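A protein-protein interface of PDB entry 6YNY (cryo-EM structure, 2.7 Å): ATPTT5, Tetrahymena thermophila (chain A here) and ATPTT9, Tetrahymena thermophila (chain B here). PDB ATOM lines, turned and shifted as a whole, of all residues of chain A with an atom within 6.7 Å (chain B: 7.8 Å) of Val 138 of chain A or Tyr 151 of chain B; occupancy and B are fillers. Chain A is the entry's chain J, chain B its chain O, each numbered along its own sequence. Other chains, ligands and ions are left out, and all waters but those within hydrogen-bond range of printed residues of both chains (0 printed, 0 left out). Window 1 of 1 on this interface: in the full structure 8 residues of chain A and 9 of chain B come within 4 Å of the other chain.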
ATOM      1  N   ASN A 131      30.885   4.983   1.541  1.00  0.00           N
ATOM      2  CA  ASN A 131      30.776   6.365   1.988  1.00  0.00           C
ATOM      3  C   ASN A 131      29.377   6.917   1.760  1.00  0.00           C
ATOM      4  O   ASN A 131      28.919   7.777   2.519  1.00  0.00           O
ATOM      5  CB  ASN A 131      31.816   7.224   1.275  1.00  0.00           C
ATOM      6  CG  ASN A 131      31.934   8.613   1.865  1.00  0.00           C
ATOM      7  OD1 ASN A 131      30.937   9.303   2.070  1.00  0.00           O
ATOM      8  ND2 ASN A 131      33.160   9.030   2.150  1.00  0.00           N
ATOM      9  N   ARG A 133      26.404   5.071   1.795  1.00  0.00           N
ATOM     10  CA  ARG A 133      25.544   4.505   2.827  1.00  0.00           C
ATOM     11  C   ARG A 133      25.819   5.141   4.178  1.00  0.00           C
ATOM     12  O   ARG A 133      24.889   5.448   4.933  1.00  0.00           O
ATOM     13  CB  ARG A 133      25.752   2.998   2.916  1.00  0.00           C
ATOM     14  CG  ARG A 133      25.376   2.220   1.681  1.00  0.00           C
ATOM     15  CD  ARG A 133      25.505   0.740   1.961  1.00  0.00           C
ATOM     16  NE  ARG A 133      24.505   0.287   2.925  1.00  0.00           N
ATOM     17  CZ  ARG A 133      24.709  -0.652   3.845  1.00  0.00           C
ATOM     18  NH1 ARG A 133      23.727  -0.985   4.667  1.00  0.00           N
ATOM     19  NH2 ARG A 133      25.888  -1.243   3.964  1.00  0.00           N
ATOM     20  N   ARG A 134      27.093   5.340   4.502  1.00  0.00           N
ATOM     21  CA  ARG A 134      27.458   5.933   5.781  1.00  0.00           C
ATOM     22  C   ARG A 134      26.914   7.349   5.898  1.00  0.00           C
ATOM     23  O   ARG A 134      26.310   7.713   6.912  1.00  0.00           O
ATOM     24  CB  ARG A 134      28.974   5.918   5.928  1.00  0.00           C
ATOM     25  CG  ARG A 134      29.479   6.316   7.284  1.00  0.00           C
ATOM     26  CD  ARG A 134      30.973   6.168   7.335  1.00  0.00           C
ATOM     27  NE  ARG A 134      31.634   7.063   6.396  1.00  0.00           N
ATOM     28  CZ  ARG A 134      32.877   6.903   5.959  1.00  0.00           C
ATOM     29  NH1 ARG A 134      33.391   7.776   5.108  1.00  0.00           N
ATOM     30  NH2 ARG A 134      33.601   5.868   6.358  1.00  0.00           N
ATOM     31  N   CYS A 135      27.119   8.165   4.865  1.00  0.00           N
ATOM     32  CA  CYS A 135      26.555   9.505   4.864  1.00  0.00           C
ATOM     33  C   CYS A 135      25.037   9.471   4.789  1.00  0.00           C
ATOM     34  O   CYS A 135      24.385  10.443   5.185  1.00  0.00           O
ATOM     35  CB  CYS A 135      27.123  10.303   3.691  1.00  0.00           C
ATOM     36  SG  CYS A 135      26.749  12.063   3.719  1.00  0.00           S
ATOM     37  N   GLN A 136      24.467   8.373   4.296  1.00  0.00           N
ATOM     38  CA  GLN A 136      23.018   8.259   4.194  1.00  0.00           C
ATOM     39  C   GLN A 136      22.390   8.049   5.565  1.00  0.00           C
ATOM     40  O   GLN A 136      21.489   8.792   5.968  1.00  0.00           O
ATOM     41  CB  GLN A 136      22.666   7.107   3.255  1.00  0.00           C
ATOM     42  CG  GLN A 136      21.223   7.041   2.828  1.00  0.00           C
ATOM     43  CD  GLN A 136      20.947   5.830   1.963  1.00  0.00           C
ATOM     44  OE1 GLN A 136      21.592   4.792   2.108  1.00  0.00           O
ATOM     45  NE2 GLN A 136      19.995   5.957   1.050  1.00  0.00           N
ATOM     46  N   MET A 137      22.860   7.039   6.300  1.00  0.00           N
ATOM     47  CA  MET A 137      22.312   6.743   7.617  1.00  0.00           C
ATOM     48  C   MET A 137      22.650   7.813   8.646  1.00  0.00           C
ATOM     49  O   MET A 137      21.985   7.886   9.684  1.00  0.00           O
ATOM     50  CB  MET A 137      22.823   5.389   8.109  1.00  0.00           C
ATOM     51  CG  MET A 137      24.320   5.327   8.299  1.00  0.00           C
ATOM     52  SD  MET A 137      24.886   3.809   9.095  1.00  0.00           S
ATOM     53  CE  MET A 137      24.535   2.592   7.833  1.00  0.00           C
ATOM     54  N   VAL A 138      23.660   8.638   8.386  1.00  0.00           N
ATOM     55  CA  VAL A 138      24.061   9.685   9.318  1.00  0.00           C
ATOM     56  C   VAL A 138      23.372  10.999   8.978  1.00  0.00           C
ATOM     57  O   VAL A 138      22.688  11.588   9.821  1.00  0.00           O
ATOM     58  CB  VAL A 138      25.589   9.858   9.315  1.00  0.00           C
ATOM     59  CG1 VAL A 138      26.001  11.018  10.198  1.00  0.00           C
ATOM     60  CG2 VAL A 138      26.261   8.591   9.771  1.00  0.00           C
ATOM     61  N   ASN A 139      23.543  11.464   7.744  1.00  0.00           N
ATOM     62  CA  ASN A 139      23.024  12.758   7.331  1.00  0.00           C
ATOM     63  C   ASN A 139      21.747  12.673   6.507  1.00  0.00           C
ATOM     64  O   ASN A 139      21.120  13.709   6.267  1.00  0.00           O
ATOM     65  CB  ASN A 139      24.085  13.512   6.525  1.00  0.00           C
ATOM     66  CG  ASN A 139      25.344  13.767   7.318  1.00  0.00           C
ATOM     67  OD1 ASN A 139      25.390  14.657   8.165  1.00  0.00           O
ATOM     68  ND2 ASN A 139      26.380  12.995   7.036  1.00  0.00           N
ATOM     69  N   GLY A 140      21.345  11.486   6.073  1.00  0.00           N
ATOM     70  CA  GLY A 140      20.152  11.338   5.270  1.00  0.00           C
ATOM     71  C   GLY A 140      20.439  11.332   3.780  1.00  0.00           C
ATOM     72  O   GLY A 140      21.517  11.703   3.309  1.00  0.00           O
ATOM     73  N   LYS A 143      21.186  14.679   1.580  1.00  0.00           N
ATOM     74  CA  LYS A 143      22.497  15.298   1.739  1.00  0.00           C
ATOM     75  C   LYS A 143      23.611  14.331   1.352  1.00  0.00           C
ATOM     76  O   LYS A 143      24.636  14.231   2.029  1.00  0.00           O
ATOM     77  CB  LYS A 143      22.690  15.796   3.168  1.00  0.00           C
ATOM     78  CG  LYS A 143      21.902  17.052   3.484  1.00  0.00           C
ATOM     79  CD  LYS A 143      22.275  17.638   4.833  1.00  0.00           C
ATOM     80  CE  LYS A 143      21.783  16.772   5.973  1.00  0.00           C
ATOM     81  NZ  LYS A 143      22.144  17.332   7.306  1.00  0.00           N
ATOM     82  N   ASN B 114      38.728   6.952  19.997  1.00  0.00           N
ATOM     83  CA  ASN B 114      38.421   7.244  18.601  1.00  0.00           C
ATOM     84  C   ASN B 114      38.537   6.004  17.727  1.00  0.00           C
ATOM     85  O   ASN B 114      37.778   5.852  16.764  1.00  0.00           O
ATOM     86  CB  ASN B 114      39.346   8.343  18.087  1.00  0.00           C
ATOM     87  CG  ASN B 114      39.243   9.614  18.901  1.00  0.00           C
ATOM     88  OD1 ASN B 114      38.713   9.613  20.011  1.00  0.00           O
ATOM     89  ND2 ASN B 114      39.755  10.706  18.354  1.00  0.00           N
ATOM     90  N   LEU B 117      35.383   3.930  18.106  1.00  0.00           N
ATOM     91  CA  LEU B 117      34.298   4.538  17.349  1.00  0.00           C
ATOM     92  C   LEU B 117      34.428   4.228  15.867  1.00  0.00           C
ATOM     93  O   LEU B 117      33.433   3.936  15.195  1.00  0.00           O
ATOM     94  CB  LEU B 117      34.288   6.047  17.571  1.00  0.00           C
ATOM     95  CG  LEU B 117      34.123   6.535  19.007  1.00  0.00           C
ATOM     96  CD1 LEU B 117      34.368   8.022  19.069  1.00  0.00           C
ATOM     97  CD2 LEU B 117      32.749   6.204  19.536  1.00  0.00           C
ATOM     98  N   ARG B 118      35.650   4.284  15.342  1.00  0.00           N
ATOM     99  CA  ARG B 118      35.854   4.014  13.927  1.00  0.00           C
ATOM    100  C   ARG B 118      35.527   2.567  13.591  1.00  0.00           C
ATOM    101  O   ARG B 118      34.931   2.286  12.545  1.00  0.00           O
ATOM    102  CB  ARG B 118      37.293   4.340  13.546  1.00  0.00           C
ATOM    103  CG  ARG B 118      37.567   4.285  12.069  1.00  0.00           C
ATOM    104  CD  ARG B 118      39.007   4.617  11.771  1.00  0.00           C
ATOM    105  NE  ARG B 118      39.921   3.655  12.371  1.00  0.00           N
ATOM    106  CZ  ARG B 118      41.241   3.704  12.249  1.00  0.00           C
ATOM    107  NH1 ARG B 118      41.809   4.667  11.546  1.00  0.00           N
ATOM    108  NH2 ARG B 118      41.993   2.786  12.832  1.00  0.00           N
ATOM    109  N   ASN B 119      35.903   1.636  14.467  1.00  0.00           N
ATOM    110  CA  ASN B 119      35.624   0.229  14.209  1.00  0.00           C
ATOM    111  C   ASN B 119      34.137  -0.075  14.302  1.00  0.00           C
ATOM    112  O   ASN B 119      33.635  -0.937  13.574  1.00  0.00           O
ATOM    113  CB  ASN B 119      36.404  -0.648  15.186  1.00  0.00           C
ATOM    114  CG  ASN B 119      37.896  -0.414  15.112  1.00  0.00           C
ATOM    115  OD1 ASN B 119      38.430  -0.065  14.060  1.00  0.00           O
ATOM    116  ND2 ASN B 119      38.579  -0.601  16.232  1.00  0.00           N
ATOM    117  N   PHE B 121      31.694   1.927  13.412  1.00  0.00           N
ATOM    118  CA  PHE B 121      31.037   2.439  12.217  1.00  0.00           C
ATOM    119  C   PHE B 121      31.352   1.634  10.964  1.00  0.00           C
ATOM    120  O   PHE B 121      30.752   1.897   9.917  1.00  0.00           O
ATOM    121  CB  PHE B 121      31.425   3.897  11.986  1.00  0.00           C
ATOM    122  CG  PHE B 121      30.559   4.874  12.712  1.00  0.00           C
ATOM    123  CD1 PHE B 121      29.487   5.467  12.077  1.00  0.00           C
ATOM    124  CD2 PHE B 121      30.813   5.201  14.027  1.00  0.00           C
ATOM    125  CE1 PHE B 121      28.690   6.365  12.739  1.00  0.00           C
ATOM    126  CE2 PHE B 121      30.017   6.099  14.693  1.00  0.00           C
ATOM    127  CZ  PHE B 121      28.955   6.682  14.050  1.00  0.00           C
ATOM    128  N   LYS B 122      32.271   0.678  11.036  1.00  0.00           N
ATOM    129  CA  LYS B 122      32.575  -0.189   9.909  1.00  0.00           C
ATOM    130  C   LYS B 122      31.661  -1.403   9.846  1.00  0.00           C
ATOM    131  O   LYS B 122      31.914  -2.314   9.053  1.00  0.00           O
ATOM    132  CB  LYS B 122      34.034  -0.637   9.968  1.00  0.00           C
ATOM    133  CG  LYS B 122      35.020   0.470   9.673  1.00  0.00           C
ATOM    134  CD  LYS B 122      36.416  -0.042   9.369  1.00  0.00           C
ATOM    135  CE  LYS B 122      37.123  -0.575  10.599  1.00  0.00           C
ATOM    136  NZ  LYS B 122      36.648  -1.929  10.997  1.00  0.00           N
ATOM    137  N   LYS B 126      22.955  -0.384  10.921  1.00  0.00           N
ATOM    138  CA  LYS B 126      22.997   0.687  11.908  1.00  0.00           C
ATOM    139  C   LYS B 126      22.712   0.164  13.309  1.00  0.00           C
ATOM    140  O   LYS B 126      23.323   0.618  14.283  1.00  0.00           O
ATOM    141  CB  LYS B 126      21.996   1.775  11.530  1.00  0.00           C
ATOM    142  CG  LYS B 126      21.967   2.952  12.474  1.00  0.00           C
ATOM    143  CD  LYS B 126      20.954   3.976  12.027  1.00  0.00           C
ATOM    144  CE  LYS B 126      20.931   5.173  12.947  1.00  0.00           C
ATOM    145  NZ  LYS B 126      19.877   6.140  12.549  1.00  0.00           N
ATOM    146  N   ILE B 129      25.784  -0.912  14.917  1.00  0.00           N
ATOM    147  CA  ILE B 129      26.667   0.176  15.319  1.00  0.00           C
ATOM    148  C   ILE B 129      26.280   0.685  16.699  1.00  0.00           C
ATOM    149  O   ILE B 129      27.126   0.831  17.587  1.00  0.00           O
ATOM    150  CB  ILE B 129      26.629   1.307  14.278  1.00  0.00           C
ATOM    151  CG1 ILE B 129      27.095   0.793  12.918  1.00  0.00           C
ATOM    152  CG2 ILE B 129      27.487   2.464  14.734  1.00  0.00           C
ATOM    153  CD1 ILE B 129      26.921   1.776  11.798  1.00  0.00           C
ATOM    154  N   PHE B 142      25.085   7.888  18.467  1.00  0.00           N
ATOM    155  CA  PHE B 142      25.376   7.717  17.049  1.00  0.00           C
ATOM    156  C   PHE B 142      25.741   9.045  16.400  1.00  0.00           C
ATOM    157  O   PHE B 142      26.793   9.171  15.762  1.00  0.00           O
ATOM    158  CB  PHE B 142      24.175   7.083  16.353  1.00  0.00           C
ATOM    159  CG  PHE B 142      24.397   6.787  14.903  1.00  0.00           C
ATOM    160  CD1 PHE B 142      24.070   7.715  13.935  1.00  0.00           C
ATOM    161  CD2 PHE B 142      24.924   5.574  14.507  1.00  0.00           C
ATOM    162  CE1 PHE B 142      24.271   7.441  12.603  1.00  0.00           C
ATOM    163  CE2 PHE B 142      25.126   5.298  13.176  1.00  0.00           C
ATOM    164  CZ  PHE B 142      24.799   6.231  12.224  1.00  0.00           C
ATOM    165  N   GLN B 143      24.881  10.052  16.550  1.00  0.00           N
ATOM    166  CA  GLN B 143      25.140  11.341  15.919  1.00  0.00           C
ATOM    167  C   GLN B 143      26.313  12.062  16.567  1.00  0.00           C
ATOM    168  O   GLN B 143      27.031  12.804  15.888  1.00  0.00           O
ATOM    169  CB  GLN B 143      23.891  12.216  15.979  1.00  0.00           C
ATOM    170  CG  GLN B 143      22.720  11.668  15.194  1.00  0.00           C
ATOM    171  CD  GLN B 143      23.013  11.558  13.715  1.00  0.00           C
ATOM    172  OE1 GLN B 143      23.900  12.233  13.193  1.00  0.00           O
ATOM    173  NE2 GLN B 143      22.273  10.698  13.028  1.00  0.00           N
ATOM    174  N   ARG B 144      26.526  11.861  17.866  1.00  0.00           N
ATOM    175  CA  ARG B 144      27.628  12.539  18.538  1.00  0.00           C
ATOM    176  C   ARG B 144      28.969  11.931  18.157  1.00  0.00           C
ATOM    177  O   ARG B 144      29.973  12.647  18.080  1.00  0.00           O
ATOM    178  CB  ARG B 144      27.433  12.477  20.049  1.00  0.00           C
ATOM    179  CG  ARG B 144      28.262  13.478  20.825  1.00  0.00           C
ATOM    180  CD  ARG B 144      28.035  13.338  22.321  1.00  0.00           C
ATOM    181  NE  ARG B 144      26.614  13.323  22.662  1.00  0.00           N
ATOM    182  CZ  ARG B 144      25.852  14.408  22.758  1.00  0.00           C
ATOM    183  NH1 ARG B 144      26.365  15.611  22.538  1.00  0.00           N
ATOM    184  NH2 ARG B 144      24.570  14.287  23.071  1.00  0.00           N
ATOM    185  N   ALA B 145      29.006  10.621  17.915  1.00  0.00           N
ATOM    186  CA  ALA B 145      30.236   9.981  17.476  1.00  0.00           C
ATOM    187  C   ALA B 145      30.521  10.243  16.006  1.00  0.00           C
ATOM    188  O   ALA B 145      31.687  10.358  15.615  1.00  0.00           O
ATOM    189  CB  ALA B 145      30.159   8.478  17.732  1.00  0.00           C
ATOM    190  N   ALA B 146      29.478  10.343  15.182  1.00  0.00           N
ATOM    191  CA  ALA B 146      29.681  10.632  13.769  1.00  0.00           C
ATOM    192  C   ALA B 146      30.242  12.030  13.560  1.00  0.00           C
ATOM    193  O   ALA B 146      30.939  12.275  12.570  1.00  0.00           O
ATOM    194  CB  ALA B 146      28.368  10.470  13.012  1.00  0.00           C
ATOM    195  N   THR B 147      29.949  12.955  14.474  1.00  0.00           N
ATOM    196  CA  THR B 147      30.497  14.301  14.364  1.00  0.00           C
ATOM    197  C   THR B 147      31.981  14.322  14.697  1.00  0.00           C
ATOM    198  O   THR B 147      32.736  15.104  14.110  1.00  0.00           O
ATOM    199  CB  THR B 147      29.733  15.252  15.282  1.00  0.00           C
ATOM    200  OG1 THR B 147      28.352  15.281  14.903  1.00  0.00           O
ATOM    201  CG2 THR B 147      30.303  16.653  15.200  1.00  0.00           C
ATOM    202  N   ILE B 148      32.412  13.476  15.631  1.00  0.00           N
ATOM    203  CA  ILE B 148      33.829  13.388  15.964  1.00  0.00           C
ATOM    204  C   ILE B 148      34.614  12.832  14.785  1.00  0.00           C
ATOM    205  O   ILE B 148      35.657  13.372  14.399  1.00  0.00           O
ATOM    206  CB  ILE B 148      34.025  12.524  17.221  1.00  0.00           C
ATOM    207  CG1 ILE B 148      33.265  13.127  18.400  1.00  0.00           C
ATOM    208  CG2 ILE B 148      35.498  12.393  17.554  1.00  0.00           C
ATOM    209  CD1 ILE B 148      33.288  12.272  19.638  1.00  0.00           C
ATOM    210  N   LEU B 149      34.124  11.743  14.197  1.00  0.00           N
ATOM    211  CA  LEU B 149      34.799  11.107  13.076  1.00  0.00           C
ATOM    212  C   LEU B 149      34.744  11.934  11.803  1.00  0.00           C
ATOM    213  O   LEU B 149      35.490  11.639  10.863  1.00  0.00           O
ATOM    214  CB  LEU B 149      34.182   9.735  12.823  1.00  0.00           C
ATOM    215  CG  LEU B 149      34.261   8.759  13.995  1.00  0.00           C
ATOM    216  CD1 LEU B 149      33.473   7.510  13.690  1.00  0.00           C
ATOM    217  CD2 LEU B 149      35.696   8.409  14.309  1.00  0.00           C
ATOM    218  N   GLY B 150      33.888  12.947  11.742  1.00  0.00           N
ATOM    219  CA  GLY B 150      33.808  13.796  10.576  1.00  0.00           C
ATOM    220  C   GLY B 150      32.889  13.301   9.488  1.00  0.00           C
ATOM    221  O   GLY B 150      33.079  13.669   8.324  1.00  0.00           O
ATOM    222  N   TYR B 151      31.899  12.483   9.825  1.00  0.00           N
ATOM    223  CA  TYR B 151      30.951  11.967   8.848  1.00  0.00           C
ATOM    224  C   TYR B 151      29.709  12.833   8.728  1.00  0.00           C
ATOM    225  O   TYR B 151      28.854  12.551   7.884  1.00  0.00           O
ATOM    226  CB  TYR B 151      30.542  10.539   9.214  1.00  0.00           C
ATOM    227  CG  TYR B 151      31.695   9.576   9.359  1.00  0.00           C
ATOM    228  CD1 TYR B 151      32.902   9.797   8.713  1.00  0.00           C
ATOM    229  CD2 TYR B 151      31.577   8.441  10.142  1.00  0.00           C
ATOM    230  CE1 TYR B 151      33.951   8.919   8.846  1.00  0.00           C
ATOM    231  CE2 TYR B 151      32.620   7.559  10.281  1.00  0.00           C
ATOM    232  CZ  TYR B 151      33.804   7.799   9.630  1.00  0.00           C
ATOM    233  OH  TYR B 151      34.845   6.915   9.771  1.00  0.00           O
ATOM    234  N   THR B 152      29.591  13.869   9.547  1.00  0.00           N
ATOM    235  CA  THR B 152      28.431  14.741   9.539  1.00  0.00           C
ATOM    236  C   THR B 152      28.678  15.954   8.653  1.00  0.00           C
ATOM    237  O   THR B 152      29.806  16.435   8.521  1.00  0.00           O
ATOM    238  CB  THR B 152      28.095  15.194  10.958  1.00  0.00           C
ATOM    239  OG1 THR B 152      27.869  14.049  11.787  1.00  0.00           O
ATOM    240  CG2 THR B 152      26.857  16.062  10.956  1.00  0.00           C
ATOM    241  N   LYS B 153      27.604  16.442   8.044  1.00  0.00           N
ATOM    242  CA  LYS B 153      27.672  17.606   7.173  1.00  0.00           C
ATOM    243  C   LYS B 153      27.471  18.893   7.963  1.00  0.00           C
ATOM    244  O   LYS B 153      26.441  19.554   7.837  1.00  0.00           O
ATOM    245  CB  LYS B 153      26.622  17.502   6.070  1.00  0.00           C
ATOM    246  CG  LYS B 153      26.762  16.271   5.196  1.00  0.00           C
ATOM    247  CD  LYS B 153      27.994  16.336   4.320  1.00  0.00           C
ATOM    248  CE  LYS B 153      28.131  15.082   3.480  1.00  0.00           C
ATOM    249  NZ  LYS B 153      29.267  15.149   2.526  1.00  0.00           N
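The backbone carbonyl oxygen (O) of Val 138 of chain A lies within hydrogen-bond range of the side-chain amide nitrogen (NE2) of Gln 143 of chain B, at 3.4 Å. O of Tyr 151 of chain B lies within hydrogen-bond range of ND2 of Asn 139 of chain A, at 2.7 Å. N of Lys 153 of chain B is in hydrogen-bond range of OD1 of Asn 139 of chain A, at 2.8 Å.
The side-chain amide nitrogen (ND2) of Asn 131 of chain A sits close to the guanidinium group (NH1) of Arg 134 of chain A. The side-chain sulfur (SG) of Cys 135 of chain A lies within hydrogen-bond range of the side-chain amide nitrogen (ND2) of Asn 139 of chain A, at 3.5 Å. O of Cys 135 of chain A sits at hydrogen-bond distance from N of Gly 140 of chain A (3.3 Å). O of Lys 143 of chain A is in hydrogen-bond range of SG of Cys 135 of chain A (3.5 Å). The backbone carbonyl oxygen of Ala 146 of chain B sits at hydrogen-bond distance from the backbone NH of Tyr 151 of chain B (2.9 Å). The side-chain hydroxyl (OG1) of Thr 152 of chain B sits at hydrogen-bond distance from the side-chain hydroxyl (OG1) of Thr 147 of chain B (3.4 Å).
Arg 134 of chain A touches Tyr 151 of chain B. Cys 135 of chain A touches Lys 153 of chain B (SG to CE, 3.3 Å). Met 137 of chain A touches Lys 126 of chain B (O to NZ, 3.96 Å). Met 137 of chain A touches Ile 129 of chain B. Met 137 of chain A touches Phe 142 of chain B (O to CE1, 3.7 Å). Val 138 of chain A touches Ala 146 of chain B. O of Tyr 151 of chain B touches CG1 of Val 138 of chain A, 3.98 Å away. Val 138 of chain A touches Thr 152 of chain B. Thr 152 of chain B touches Asn 139 of chain A. Lys 153 of chain B touches Lys 143 of chain A.
Of the printed residues of chain B, Val 138 of chain A touches Phe 142, Gln 143, Ala 146, Tyr 151 and Thr 152. Of the printed residues of chain A, Tyr 151 of chain B touches Arg 134 (3.7 Å), Val 138 (3.98 Å) and Asn 139 (2.7 Å). Of the printed residues of chain A, Ile 129 of chain B touches Met 137 (3.9 Å). Printed residues of chain B within 4 Å of Cys 135 of chain A: Lys 153. Printed residues of chain B within 4 Å of Asn 139 of chain A: Tyr 151 (2.7 Å), Thr 152 (3.3 Å) and Lys 153 (2.8 Å). Of the printed residues of chain A, Ala 146 of chain B touches Val 138. The nearest printed residue of chain B that does not touch Val 138 of chain A is Phe 121 of chain B (4.4 Å). The nearest printed residue of chain A that does not touch Tyr 151 of chain B is Cys 135 of chain A (4.7 Å).
Hydrophobic or aromatic side chains of chain B that line the printed part of chain A: Ile 129, Phe 142, Ala 146 and Tyr 151. Of the 10 printed residues of chain A, 6 touch a printed residue of chain B. Printed residues of chain A that touch a printed residue of chain B: Arg 134, Cys 135, Met 137, Val 138, Asn 139 and Lys 143. Hydrophobic or aromatic side chains of chain A within 4 Å of the printed part of chain B: Met 137 and Val 138. Among the printed residues, no Asp or Glu carboxylate lies within 4 Å of a Lys or Arg side-chain nitrogen of the other chain.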
